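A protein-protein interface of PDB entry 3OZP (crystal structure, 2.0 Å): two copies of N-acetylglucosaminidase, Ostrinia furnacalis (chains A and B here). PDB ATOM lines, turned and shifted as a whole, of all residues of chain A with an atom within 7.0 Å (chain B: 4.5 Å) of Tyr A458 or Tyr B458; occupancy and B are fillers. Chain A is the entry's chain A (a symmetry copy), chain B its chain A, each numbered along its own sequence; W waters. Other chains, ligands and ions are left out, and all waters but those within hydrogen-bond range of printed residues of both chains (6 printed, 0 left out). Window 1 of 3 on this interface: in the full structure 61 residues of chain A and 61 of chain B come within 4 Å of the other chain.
Printed residues of chain B within 4 Å of Pro A471: Asn B466. Of the printed residues of chain B, Arg A514 touches Glu B556 (2.7 Å). Printed residues of chain B within 4 Å of Ser A557: Gln B505. Of the printed residues of chain A, Gly B457 touches Tyr A472. Of the printed residues of chain A, Tyr B458 touches Tyr A458 and Tyr A472. Of the printed residues of chain A, Asn B466 touches Pro A471 and Tyr A472. Printed residues of chain A within 4 Å of Arg B514: Glu A556 (2.7 Å). The nearest residue of chain B that does not touch Tyr A458 is Glu B556 (4.2 Å). The nearest residue of chain A that does not touch Tyr B458 is Glu A556 (4.2 Å). The nearest printed residue of chain A that does not touch Glu B556 is Gln A505 (4.1 Å).
ND2 of Asn B466 sits at hydrogen-bond distance from O of Tyr A472, 2.9 Å away. O of Tyr B472 lies within hydrogen-bond range of ND2 of Asn A466 (2.9 Å). The side-chain carboxylate (OE2) of Glu A556 lies within salt-bridge range of the guanidinium group (NH2) of Arg B514 (2.7 Å). OE2 of Glu B556 lies within salt-bridge range of NH2 of Arg A514, 2.7 Å away.
Gly A457 touches Tyr B472. Tyr A458 touches Tyr B458. Tyr A458 touches Tyr B472. Gly A459 touches Tyr B472 (N to CD1, 3.6 Å). Pro A471 touches Asn B466. Tyr A472 touches Gly B457. Tyr A472 touches Tyr B458 (CD1 to CA, 3.7 Å). N of Gly B459 touches CD1 of Tyr A472 (3.6 Å). CA of Glu B556 touches CG2 of Thr A510, 3.8 Å away. Gln B505 touches Ser A557 (C to CB, 3.4 Å).
N of Gly B457 lies within hydrogen-bond range of OD1 of Asn B467 (3.0 Å). The guanidinium group (NH2) of Arg B514 is in hydrogen-bond range of the backbone carbonyl oxygen (O) of Gln B505, 2.9 Å away. O of Gly A457 is in hydrogen-bond range of ND2 of Asn A466 (3.3 Å). The guanidinium group of Arg A514 sits at hydrogen-bond distance from the side-chain hydroxyl of Tyr A458, at 3.3 Å. O of Gln A505 sits at hydrogen-bond distance from NH2 of Arg A514 (2.9 Å). O of Arg A514 lies within hydrogen-bond range of NH2 of Arg A518.
Gly A457 touches Tyr B472, and with the chains exchanged Tyr A472 touches Gly B457. Tyr B458 touches its own counterpart, Tyr A458. Asn A466 touches Tyr B472, and with the chains exchanged Tyr A472 touches Asn B466. Arg A514 touches Glu B556, and with the chains exchanged Glu A556 touches Arg B514. 13 positions are printed for both chains. Of the 14 pairs that touch across the chains among the printed residues, 11 have their exchanged pair printed and touching as well.
Water W1 lies within hydrogen-bond range of OE2 of Glu B556, O of Gln A505, NH2 of Arg A514 and OG1 of Thr A510. Water W4 lies within hydrogen-bond range of the backbone carbonyl oxygen (O) of Gly A457, the backbone NH (N) of Tyr B472 and the side-chain amide nitrogen (ND2) of Asn A466. Water W5 lies within hydrogen-bond range of the side-chain amide oxygen of Asn B466 (2.8 Å) and the backbone carbonyl oxygen of Tyr A472 (3.1 Å). Water W3 lies within hydrogen-bond range of OD1 of Asn A466 and O of Tyr B472.
Of the 13 printed residues of chain B, 8 touch a printed residue of chain A. Printed residues of chain B that touch a printed residue of chain A: Gly B457, Tyr B458, Gly B459, Asn B466, Tyr B472, Gln B505, Arg B514 and Glu B556. Hydrophobic or aromatic side chains of chain B that line the printed part of chain A: Tyr B458 and Tyr B472. Among the printed residues, 14 pairs touch across the chains. Among the printed residues, Asp or Glu carboxylates within 4 Å of a Lys or Arg side-chain nitrogen of the other chain: Arg A514 with Glu B556 and Glu A556 with Arg B514.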
ATOM      1  N   PHE A 454     -15.654  -2.621  -4.486  1.00  0.00           N
ATOM      2  CA  PHE A 454     -14.794  -1.662  -3.785  1.00  0.00           C
ATOM      3  C   PHE A 454     -13.307  -1.934  -3.992  1.00  0.00           C
ATOM      4  O   PHE A 454     -12.457  -1.129  -3.599  1.00  0.00           O
ATOM      5  CB  PHE A 454     -15.145  -1.643  -2.296  1.00  0.00           C
ATOM      6  CG  PHE A 454     -16.346  -0.783  -1.958  1.00  0.00           C
ATOM      7  CD1 PHE A 454     -17.306  -0.465  -2.925  1.00  0.00           C
ATOM      8  CD2 PHE A 454     -16.530  -0.319  -0.660  1.00  0.00           C
ATOM      9  CE1 PHE A 454     -18.419   0.326  -2.601  1.00  0.00           C
ATOM     10  CE2 PHE A 454     -17.636   0.469  -0.328  1.00  0.00           C
ATOM     11  CZ  PHE A 454     -18.581   0.793  -1.302  1.00  0.00           C
ATOM     12  N   ASP A 455     -13.006  -3.057  -4.637  1.00  0.00           N
ATOM     13  CA  ASP A 455     -11.633  -3.438  -4.949  1.00  0.00           C
ATOM     14  C   ASP A 455     -11.111  -2.815  -6.249  1.00  0.00           C
ATOM     15  O   ASP A 455      -9.895  -2.764  -6.470  1.00  0.00           O
ATOM     16  CB  ASP A 455     -11.505  -4.967  -4.994  1.00  0.00           C
ATOM     17  CG  ASP A 455     -12.463  -5.616  -5.989  1.00  0.00           C
ATOM     18  OD1 ASP A 455     -13.648  -5.218  -6.056  1.00  0.00           O
ATOM     19  OD2 ASP A 455     -12.032  -6.539  -6.706  1.00  0.00           O
ATOM     20  N   CYS A 456     -12.026  -2.337  -7.099  1.00  0.00           N
ATOM     21  CA  CYS A 456     -11.674  -1.801  -8.421  1.00  0.00           C
ATOM     22  C   CYS A 456     -10.817  -0.541  -8.378  1.00  0.00           C
ATOM     23  O   CYS A 456     -10.988   0.311  -7.501  1.00  0.00           O
ATOM     24  CB  CYS A 456     -12.935  -1.459  -9.226  1.00  0.00           C
ATOM     25  SG  CYS A 456     -14.184  -2.737  -9.317  1.00  0.00           S
ATOM     26  N   GLY A 457      -9.917  -0.421  -9.352  1.00  0.00           N
ATOM     27  CA  GLY A 457      -9.209   0.834  -9.591  1.00  0.00           C
ATOM     28  C   GLY A 457      -7.708   0.814  -9.389  1.00  0.00           C
ATOM     29  O   GLY A 457      -6.993   1.663  -9.930  1.00  0.00           O
ATOM     30  N   TYR A 458      -7.220  -0.147  -8.618  1.00  0.00           N
ATOM     31  CA  TYR A 458      -5.803  -0.169  -8.258  1.00  0.00           C
ATOM     32  C   TYR A 458      -4.949  -0.822  -9.340  1.00  0.00           C
ATOM     33  O   TYR A 458      -5.458  -1.158 -10.411  1.00  0.00           O
ATOM     34  CB  TYR A 458      -5.619  -0.824  -6.891  1.00  0.00           C
ATOM     35  CG  TYR A 458      -6.324  -0.036  -5.817  1.00  0.00           C
ATOM     36  CD1 TYR A 458      -5.680   1.014  -5.167  1.00  0.00           C
ATOM     37  CD2 TYR A 458      -7.650  -0.306  -5.487  1.00  0.00           C
ATOM     38  CE1 TYR A 458      -6.334   1.760  -4.193  1.00  0.00           C
ATOM     39  CE2 TYR A 458      -8.312   0.432  -4.522  1.00  0.00           C
ATOM     40  CZ  TYR A 458      -7.645   1.460  -3.883  1.00  0.00           C
ATOM     41  OH  TYR A 458      -8.291   2.188  -2.915  1.00  0.00           O
ATOM     42  N   GLY A 459      -3.655  -0.975  -9.078  1.00  0.00           N
ATOM     43  CA  GLY A 459      -2.756  -1.586 -10.053  1.00  0.00           C
ATOM     44  C   GLY A 459      -3.183  -3.011 -10.344  1.00  0.00           C
ATOM     45  O   GLY A 459      -3.965  -3.596  -9.587  1.00  0.00           O
ATOM     46  N   ALA A 460      -2.697  -3.565 -11.452  1.00  0.00           N
ATOM     47  CA  ALA A 460      -2.878  -4.988 -11.728  1.00  0.00           C
ATOM     48  C   ALA A 460      -2.169  -5.800 -10.652  1.00  0.00           C
ATOM     49  O   ALA A 460      -1.135  -5.368 -10.132  1.00  0.00           O
ATOM     50  CB  ALA A 460      -2.322  -5.334 -13.102  1.00  0.00           C
ATOM     51  N   TRP A 461      -2.732  -6.952 -10.299  1.00  0.00           N
ATOM     52  CA  TRP A 461      -2.038  -7.896  -9.416  1.00  0.00           C
ATOM     53  C   TRP A 461      -1.466  -9.091 -10.189  1.00  0.00           C
ATOM     54  O   TRP A 461      -0.622  -9.823  -9.674  1.00  0.00           O
ATOM     55  CB  TRP A 461      -2.910  -8.328  -8.232  1.00  0.00           C
ATOM     56  CG  TRP A 461      -4.103  -9.186  -8.560  1.00  0.00           C
ATOM     57  CD1 TRP A 461      -5.353  -8.756  -8.904  1.00  0.00           C
ATOM     58  CD2 TRP A 461      -4.166 -10.619  -8.535  1.00  0.00           C
ATOM     59  NE1 TRP A 461      -6.186  -9.831  -9.106  1.00  0.00           N
ATOM     60  CE2 TRP A 461      -5.483 -10.986  -8.887  1.00  0.00           C
ATOM     61  CE3 TRP A 461      -3.232 -11.629  -8.258  1.00  0.00           C
ATOM     62  CZ2 TRP A 461      -5.894 -12.322  -8.969  1.00  0.00           C
ATOM     63  CZ3 TRP A 461      -3.642 -12.963  -8.332  1.00  0.00           C
ATOM     64  CH2 TRP A 461      -4.963 -13.294  -8.687  1.00  0.00           C
ATOM     65  N   GLY A 465      -0.530  -2.541 -15.524  1.00  0.00           N
ATOM     66  CA  GLY A 465      -1.740  -1.764 -15.780  1.00  0.00           C
ATOM     67  C   GLY A 465      -2.577  -1.649 -14.518  1.00  0.00           C
ATOM     68  O   GLY A 465      -2.038  -1.471 -13.420  1.00  0.00           O
ATOM     69  N   ASN A 466      -3.892  -1.756 -14.676  1.00  0.00           N
ATOM     70  CA  ASN A 466      -4.826  -1.655 -13.559  1.00  0.00           C
ATOM     71  C   ASN A 466      -5.665  -2.918 -13.430  1.00  0.00           C
ATOM     72  O   ASN A 466      -5.769  -3.684 -14.387  1.00  0.00           O
ATOM     73  CB  ASN A 466      -5.721  -0.421 -13.735  1.00  0.00           C
ATOM     74  CG  ASN A 466      -4.948   0.878 -13.603  1.00  0.00           C
ATOM     75  OD1 ASN A 466      -4.528   1.463 -14.599  1.00  0.00           O
ATOM     76  ND2 ASN A 466      -4.736   1.324 -12.367  1.00  0.00           N
ATOM     77  N   ASN A 467      -6.260  -3.145 -12.255  1.00  0.00           N
ATOM     78  CA  ASN A 467      -7.089  -4.341 -12.059  1.00  0.00           C
ATOM     79  C   ASN A 467      -8.371  -4.332 -12.921  1.00  0.00           C
ATOM     80  O   ASN A 467      -8.759  -3.284 -13.444  1.00  0.00           O
ATOM     81  CB  ASN A 467      -7.347  -4.643 -10.570  1.00  0.00           C
ATOM     82  CG  ASN A 467      -8.241  -3.616  -9.884  1.00  0.00           C
ATOM     83  OD1 ASN A 467      -9.137  -3.030 -10.492  1.00  0.00           O
ATOM     84  ND2 ASN A 467      -8.017  -3.426  -8.587  1.00  0.00           N
ATOM     85  N   TRP A 468      -9.010  -5.497 -13.046  1.00  0.00           N
ATOM     86  CA  TRP A 468     -10.004  -5.770 -14.100  1.00  0.00           C
ATOM     87  C   TRP A 468     -11.193  -4.815 -14.179  1.00  0.00           C
ATOM     88  O   TRP A 468     -11.666  -4.500 -15.280  1.00  0.00           O
ATOM     89  CB  TRP A 468     -10.510  -7.226 -14.021  1.00  0.00           C
ATOM     90  CG  TRP A 468     -11.595  -7.466 -12.993  1.00  0.00           C
ATOM     91  CD1 TRP A 468     -11.421  -7.793 -11.675  1.00  0.00           C
ATOM     92  CD2 TRP A 468     -13.016  -7.405 -13.204  1.00  0.00           C
ATOM     93  NE1 TRP A 468     -12.639  -7.934 -11.055  1.00  0.00           N
ATOM     94  CE2 TRP A 468     -13.634  -7.700 -11.968  1.00  0.00           C
ATOM     95  CE3 TRP A 468     -13.824  -7.120 -14.316  1.00  0.00           C
ATOM     96  CZ2 TRP A 468     -15.025  -7.730 -11.814  1.00  0.00           C
ATOM     97  CZ3 TRP A 468     -15.211  -7.150 -14.161  1.00  0.00           C
ATOM     98  CH2 TRP A 468     -15.794  -7.451 -12.919  1.00  0.00           C
ATOM     99  N   SER A 470     -11.411  -1.670 -12.917  1.00  0.00           N
ATOM    100  CA  SER A 470     -11.065  -0.246 -12.916  1.00  0.00           C
ATOM    101  C   SER A 470     -11.966   0.493 -13.913  1.00  0.00           C
ATOM    102  O   SER A 470     -12.412  -0.109 -14.897  1.00  0.00           O
ATOM    103  CB  SER A 470      -9.590  -0.051 -13.273  1.00  0.00           C
ATOM    104  OG  SER A 470      -8.752  -0.698 -12.331  1.00  0.00           O
ATOM    105  N   PRO A 471     -12.238   1.794 -13.678  1.00  0.00           N
ATOM    106  CA  PRO A 471     -11.661   2.697 -12.673  1.00  0.00           C
ATOM    107  C   PRO A 471     -12.192   2.532 -11.240  1.00  0.00           C
ATOM    108  O   PRO A 471     -13.158   1.802 -10.998  1.00  0.00           O
ATOM    109  CB  PRO A 471     -12.010   4.088 -13.216  1.00  0.00           C
ATOM    110  CG  PRO A 471     -13.281   3.882 -13.977  1.00  0.00           C
ATOM    111  CD  PRO A 471     -13.236   2.481 -14.527  1.00  0.00           C
ATOM    112  N   TYR A 472     -11.528   3.210 -10.308  1.00  0.00           N
ATOM    113  CA  TYR A 472     -11.951   3.283  -8.915  1.00  0.00           C
ATOM    114  C   TYR A 472     -13.324   3.935  -8.826  1.00  0.00           C
ATOM    115  O   TYR A 472     -13.574   4.965  -9.456  1.00  0.00           O
ATOM    116  CB  TYR A 472     -10.921   4.084  -8.121  1.00  0.00           C
ATOM    117  CG  TYR A 472     -11.201   4.251  -6.642  1.00  0.00           C
ATOM    118  CD1 TYR A 472     -11.871   5.378  -6.163  1.00  0.00           C
ATOM    119  CD2 TYR A 472     -10.758   3.306  -5.718  1.00  0.00           C
ATOM    120  CE1 TYR A 472     -12.113   5.549  -4.798  1.00  0.00           C
ATOM    121  CE2 TYR A 472     -10.991   3.469  -4.349  1.00  0.00           C
ATOM    122  CZ  TYR A 472     -11.665   4.593  -3.900  1.00  0.00           C
ATOM    123  OH  TYR A 472     -11.898   4.761  -2.552  1.00  0.00           O
ATOM    124  N   ILE A 473     -14.206   3.324  -8.045  1.00  0.00           N
ATOM    125  CA  ILE A 473     -15.578   3.793  -7.923  1.00  0.00           C
ATOM    126  C   ILE A 473     -15.678   4.777  -6.766  1.00  0.00           C
ATOM    127  O   ILE A 473     -15.530   4.388  -5.608  1.00  0.00           O
ATOM    128  CB  ILE A 473     -16.556   2.618  -7.707  1.00  0.00           C
ATOM    129  CG1 ILE A 473     -16.415   1.590  -8.839  1.00  0.00           C
ATOM    130  CG2 ILE A 473     -18.003   3.131  -7.564  1.00  0.00           C
ATOM    131  CD1 ILE A 473     -17.132   0.276  -8.593  1.00  0.00           C
ATOM    132  N   GLY A 474     -15.917   6.049  -7.089  1.00  0.00           N
ATOM    133  CA  GLY A 474     -16.090   7.088  -6.072  1.00  0.00           C
ATOM    134  C   GLY A 474     -17.413   6.941  -5.342  1.00  0.00           C
ATOM    135  O   GLY A 474     -18.345   6.331  -5.868  1.00  0.00           O
ATOM    136  N   GLN A 505      -6.071  -7.564  -3.346  1.00  0.00           N
ATOM    137  CA  GLN A 505      -5.246  -6.387  -3.082  1.00  0.00           C
ATOM    138  C   GLN A 505      -5.734  -5.610  -1.858  1.00  0.00           C
ATOM    139  O   GLN A 505      -5.661  -4.377  -1.816  1.00  0.00           O
ATOM    140  CB  GLN A 505      -5.230  -5.476  -4.310  1.00  0.00           C
ATOM    141  CG  GLN A 505      -4.633  -6.118  -5.553  1.00  0.00           C
ATOM    142  CD  GLN A 505      -4.694  -5.205  -6.739  1.00  0.00           C
ATOM    143  OE1 GLN A 505      -3.720  -4.530  -7.064  1.00  0.00           O
ATOM    144  NE2 GLN A 505      -5.845  -5.158  -7.389  1.00  0.00           N
ATOM    145  N   THR A 510      -5.502  -2.245   4.899  1.00  0.00           N
ATOM    146  CA  THR A 510      -6.182  -1.404   3.893  1.00  0.00           C
ATOM    147  C   THR A 510      -7.698  -1.434   4.004  1.00  0.00           C
ATOM    148  O   THR A 510      -8.403  -0.718   3.292  1.00  0.00           O
ATOM    149  CB  THR A 510      -5.811  -1.838   2.462  1.00  0.00           C
ATOM    150  OG1 THR A 510      -6.206  -3.200   2.267  1.00  0.00           O
ATOM    151  CG2 THR A 510      -4.303  -1.706   2.236  1.00  0.00           C
ATOM    152  N   GLY A 513      -9.662   1.999   4.692  1.00  0.00           N
ATOM    153  CA  GLY A 513      -9.665   2.859   3.505  1.00  0.00           C
ATOM    154  C   GLY A 513     -10.542   2.344   2.379  1.00  0.00           C
ATOM    155  O   GLY A 513     -11.251   3.123   1.734  1.00  0.00           O
ATOM    156  N   ARG A 514     -10.499   1.035   2.147  1.00  0.00           N
ATOM    157  CA  ARG A 514     -11.333   0.395   1.129  1.00  0.00           C
ATOM    158  C   ARG A 514     -12.832   0.591   1.375  1.00  0.00           C
ATOM    159  O   ARG A 514     -13.592   0.874   0.445  1.00  0.00           O
ATOM    160  CB  ARG A 514     -11.022  -1.105   1.029  1.00  0.00           C
ATOM    161  CG  ARG A 514      -9.684  -1.463   0.368  1.00  0.00           C
ATOM    162  CD  ARG A 514      -9.632  -0.998  -1.084  1.00  0.00           C
ATOM    163  NE  ARG A 514      -8.478  -1.529  -1.812  1.00  0.00           N
ATOM    164  CZ  ARG A 514      -7.235  -1.057  -1.727  1.00  0.00           C
ATOM    165  NH1 ARG A 514      -6.939  -0.032  -0.934  1.00  0.00           N
ATOM    166  NH2 ARG A 514      -6.276  -1.615  -2.454  1.00  0.00           N
ATOM    167  N   ARG A 518     -16.960   5.138   1.644  1.00  0.00           N
ATOM    168  CA  ARG A 518     -17.797   4.671   0.528  1.00  0.00           C
ATOM    169  C   ARG A 518     -18.998   3.802   0.918  1.00  0.00           C
ATOM    170  O   ARG A 518     -20.096   3.995   0.384  1.00  0.00           O
ATOM    171  CB  ARG A 518     -16.951   3.991  -0.555  1.00  0.00           C
ATOM    172  CG  ARG A 518     -16.140   4.970  -1.395  1.00  0.00           C
ATOM    173  CD  ARG A 518     -15.394   4.269  -2.519  1.00  0.00           C
ATOM    174  NE  ARG A 518     -14.542   3.172  -2.052  1.00  0.00           N
ATOM    175  CZ  ARG A 518     -13.992   2.257  -2.851  1.00  0.00           C
ATOM    176  NH1 ARG A 518     -14.195   2.298  -4.165  1.00  0.00           N
ATOM    177  NH2 ARG A 518     -13.229   1.301  -2.335  1.00  0.00           N
ATOM    178  N   GLU A 556     -10.884   6.814   4.012  1.00  0.00           N
ATOM    179  CA  GLU A 556     -10.431   7.590   2.862  1.00  0.00           C
ATOM    180  C   GLU A 556     -10.777   9.061   3.041  1.00  0.00           C
ATOM    181  O   GLU A 556     -11.793   9.401   3.665  1.00  0.00           O
ATOM    182  CB  GLU A 556     -11.061   7.066   1.570  1.00  0.00           C
ATOM    183  CG  GLU A 556     -10.239   5.988   0.863  1.00  0.00           C
ATOM    184  CD  GLU A 556      -8.903   6.499   0.347  1.00  0.00           C
ATOM    185  OE1 GLU A 556      -7.896   5.783   0.491  1.00  0.00           O
ATOM    186  OE2 GLU A 556      -8.855   7.620  -0.201  1.00  0.00           O
ATOM    187  N   SER A 557      -9.919   9.925   2.506  1.00  0.00           N
ATOM    188  CA  SER A 557     -10.171  11.359   2.455  1.00  0.00           C
ATOM    189  C   SER A 557     -10.873  11.676   1.138  1.00  0.00           C
ATOM    190  O   SER A 557     -10.452  11.212   0.079  1.00  0.00           O
ATOM    191  CB  SER A 557      -8.857  12.137   2.575  1.00  0.00           C
ATOM    192  OG  SER A 557      -9.033  13.520   2.325  1.00  0.00           O
ATOM    193  N   ASP B 455      -1.330  10.647  -5.924  1.00  0.00           N
ATOM    194  CA  ASP B 455      -2.705  11.029  -5.622  1.00  0.00           C
ATOM    195  C   ASP B 455      -3.708  10.592  -6.696  1.00  0.00           C
ATOM    196  O   ASP B 455      -4.916  10.538  -6.435  1.00  0.00           O
ATOM    197  CB  ASP B 455      -2.794  12.543  -5.384  1.00  0.00           C
ATOM    198  CG  ASP B 455      -2.275  13.362  -6.562  1.00  0.00           C
ATOM    199  OD1 ASP B 455      -1.222  13.015  -7.141  1.00  0.00           O
ATOM    200  OD2 ASP B 455      -2.923  14.369  -6.909  1.00  0.00           O
ATOM    201  N   CYS B 456      -3.207  10.275  -7.894  1.00  0.00           N
ATOM    202  CA  CYS B 456      -4.059   9.933  -9.042  1.00  0.00           C
ATOM    203  C   CYS B 456      -4.871   8.655  -8.860  1.00  0.00           C
ATOM    204  O   CYS B 456      -4.400   7.686  -8.255  1.00  0.00           O
ATOM    205  CB  CYS B 456      -3.218   9.754 -10.313  1.00  0.00           C
ATOM    206  SG  CYS B 456      -2.065  11.068 -10.687  1.00  0.00           S
ATOM    207  N   GLY B 457      -6.081   8.655  -9.416  1.00  0.00           N
ATOM    208  CA  GLY B 457      -6.864   7.429  -9.548  1.00  0.00           C
ATOM    209  C   GLY B 457      -8.168   7.373  -8.781  1.00  0.00           C
ATOM    210  O   GLY B 457      -9.063   6.594  -9.124  1.00  0.00           O
ATOM    211  N   TYR B 458      -8.291   8.193  -7.747  1.00  0.00           N
ATOM    212  CA  TYR B 458      -9.457   8.117  -6.868  1.00  0.00           C
ATOM    213  C   TYR B 458     -10.643   8.899  -7.425  1.00  0.00           C
ATOM    214  O   TYR B 458     -10.578   9.406  -8.546  1.00  0.00           O
ATOM    215  CB  TYR B 458      -9.079   8.554  -5.454  1.00  0.00           C
ATOM    216  CG  TYR B 458      -8.038   7.635  -4.869  1.00  0.00           C
ATOM    217  CD1 TYR B 458      -8.411   6.481  -4.184  1.00  0.00           C
ATOM    218  CD2 TYR B 458      -6.679   7.894  -5.041  1.00  0.00           C
ATOM    219  CE1 TYR B 458      -7.455   5.618  -3.664  1.00  0.00           C
ATOM    220  CE2 TYR B 458      -5.719   7.039  -4.528  1.00  0.00           C
ATOM    221  CZ  TYR B 458      -6.117   5.908  -3.843  1.00  0.00           C
ATOM    222  OH  TYR B 458      -5.170   5.062  -3.321  1.00  0.00           O
ATOM    223  N   GLY B 459     -11.730   8.972  -6.662  1.00  0.00           N
ATOM    224  CA  GLY B 459     -12.917   9.694  -7.111  1.00  0.00           C
ATOM    225  C   GLY B 459     -12.592  11.159  -7.327  1.00  0.00           C
ATOM    226  O   GLY B 459     -11.562  11.648  -6.853  1.00  0.00           O
ATOM    227  N   ALA B 460     -13.452  11.858  -8.064  1.00  0.00           N
ATOM    228  CA  ALA B 460     -13.349  13.311  -8.173  1.00  0.00           C
ATOM    229  C   ALA B 460     -13.562  13.930  -6.797  1.00  0.00           C
ATOM    230  O   ALA B 460     -14.327  13.395  -5.989  1.00  0.00           O
ATOM    231  CB  ALA B 460     -14.382  13.842  -9.155  1.00  0.00           C
ATOM    232  N   ASN B 466     -13.653  10.589 -11.732  1.00  0.00           N
ATOM    233  CA  ASN B 466     -12.362  10.351 -11.091  1.00  0.00           C
ATOM    234  C   ASN B 466     -11.501  11.605 -11.108  1.00  0.00           C
ATOM    235  O   ASN B 466     -11.752  12.509 -11.905  1.00  0.00           O
ATOM    236  CB  ASN B 466     -11.643   9.185 -11.783  1.00  0.00           C
ATOM    237  CG  ASN B 466     -12.344   7.858 -11.558  1.00  0.00           C
ATOM    238  OD1 ASN B 466     -13.134   7.417 -12.390  1.00  0.00           O
ATOM    239  ND2 ASN B 466     -12.075   7.225 -10.417  1.00  0.00           N
ATOM    240  N   ASN B 467     -10.491  11.672 -10.235  1.00  0.00           N
ATOM    241  CA  ASN B 467      -9.615  12.849 -10.200  1.00  0.00           C
ATOM    242  C   ASN B 467      -8.768  13.009 -11.480  1.00  0.00           C
ATOM    243  O   ASN B 467      -8.643  12.063 -12.263  1.00  0.00           O
ATOM    244  CB  ASN B 467      -8.792  12.932  -8.898  1.00  0.00           C
ATOM    245  CG  ASN B 467      -7.734  11.842  -8.773  1.00  0.00           C
ATOM    246  OD1 ASN B 467      -7.162  11.381  -9.761  1.00  0.00           O
ATOM    247  ND2 ASN B 467      -7.445  11.453  -7.536  1.00  0.00           N
ATOM    248  N   SER B 470      -6.044  10.469 -13.051  1.00  0.00           N
ATOM    249  CA  SER B 470      -6.406   9.051 -13.129  1.00  0.00           C
ATOM    250  C   SER B 470      -5.984   8.498 -14.496  1.00  0.00           C
ATOM    251  O   SER B 470      -5.935   9.254 -15.474  1.00  0.00           O
ATOM    252  CB  SER B 470      -7.909   8.867 -12.914  1.00  0.00           C
ATOM    253  OG  SER B 470      -8.298   9.340 -11.635  1.00  0.00           O
ATOM    254  N   TYR B 472      -5.075   5.259 -11.454  1.00  0.00           N
ATOM    255  CA  TYR B 472      -4.149   4.991 -10.361  1.00  0.00           C
ATOM    256  C   TYR B 472      -2.869   4.375 -10.908  1.00  0.00           C
ATOM    257  O   TYR B 472      -2.913   3.459 -11.732  1.00  0.00           O
ATOM    258  CB  TYR B 472      -4.816   4.049  -9.360  1.00  0.00           C
ATOM    259  CG  TYR B 472      -3.991   3.671  -8.148  1.00  0.00           C
ATOM    260  CD1 TYR B 472      -3.222   2.505  -8.139  1.00  0.00           C
ATOM    261  CD2 TYR B 472      -4.014   4.453  -6.993  1.00  0.00           C
ATOM    262  CE1 TYR B 472      -2.477   2.140  -7.016  1.00  0.00           C
ATOM    263  CE2 TYR B 472      -3.274   4.094  -5.862  1.00  0.00           C
ATOM    264  CZ  TYR B 472      -2.514   2.936  -5.883  1.00  0.00           C
ATOM    265  OH  TYR B 472      -1.783   2.575  -4.771  1.00  0.00           O
ATOM    266  N   GLN B 505      -7.087  14.698  -1.394  1.00  0.00           N
ATOM    267  CA  GLN B 505      -7.781  13.469  -1.011  1.00  0.00           C
ATOM    268  C   GLN B 505      -6.881  12.533  -0.202  1.00  0.00           C
ATOM    269  O   GLN B 505      -6.970  11.306  -0.320  1.00  0.00           O
ATOM    270  CB  GLN B 505      -8.298  12.753  -2.258  1.00  0.00           C
ATOM    271  CG  GLN B 505      -9.309  13.555  -3.063  1.00  0.00           C
ATOM    272  CD  GLN B 505      -9.739  12.833  -4.302  1.00  0.00           C
ATOM    273  OE1 GLN B 505     -10.783  12.185  -4.322  1.00  0.00           O
ATOM    274  NE2 GLN B 505      -8.932  12.919  -5.345  1.00  0.00           N
ATOM    275  N   ARG B 514      -1.143   5.511   0.604  1.00  0.00           N
ATOM    276  CA  ARG B 514      -0.748   6.321  -0.550  1.00  0.00           C
ATOM    277  C   ARG B 514       0.723   6.136  -0.933  1.00  0.00           C
ATOM    278  O   ARG B 514       1.056   6.018  -2.117  1.00  0.00           O
ATOM    279  CB  ARG B 514      -1.027   7.809  -0.294  1.00  0.00           C
ATOM    280  CG  ARG B 514      -2.505   8.221  -0.326  1.00  0.00           C
ATOM    281  CD  ARG B 514      -3.129   7.978  -1.696  1.00  0.00           C
ATOM    282  NE  ARG B 514      -4.458   8.576  -1.833  1.00  0.00           N
ATOM    283  CZ  ARG B 514      -5.585   8.059  -1.345  1.00  0.00           C
ATOM    284  NH1 ARG B 514      -5.582   6.918  -0.664  1.00  0.00           N
ATOM    285  NH2 ARG B 514      -6.733   8.691  -1.553  1.00  0.00           N
ATOM    286  N   GLU B 556      -0.242  -0.468   1.285  1.00  0.00           N
ATOM    287  CA  GLU B 556      -1.128  -1.077   0.299  1.00  0.00           C
ATOM    288  C   GLU B 556      -0.783  -2.546   0.107  1.00  0.00           C
ATOM    289  O   GLU B 556       0.383  -2.945   0.231  1.00  0.00           O
ATOM    290  CB  GLU B 556      -1.030  -0.346  -1.042  1.00  0.00           C
ATOM    291  CG  GLU B 556      -2.028   0.800  -1.206  1.00  0.00           C
ATOM    292  CD  GLU B 556      -3.476   0.332  -1.236  1.00  0.00           C
ATOM    293  OE1 GLU B 556      -4.326   0.988  -0.608  1.00  0.00           O
ATOM    294  OE2 GLU B 556      -3.765  -0.695  -1.884  1.00  0.00           O
HETATM  295  O   HOH W   1      -4.441  -2.646  -0.550  1.00  0.00           O
HETATM  296  O   HOH W   2      -7.657   9.369   1.045  1.00  0.00           O
HETATM  297  O   HOH W   3      -1.981   2.732 -14.614  1.00  0.00           O
HETATM  298  O   HOH W   4      -7.424   3.481 -11.812  1.00  0.00           O
HETATM  299  O   HOH W   5     -15.526   6.087 -11.609  1.00  0.00           O
HETATM  300  O   HOH W   6      -9.448   5.092 -11.275  1.00  0.00           O
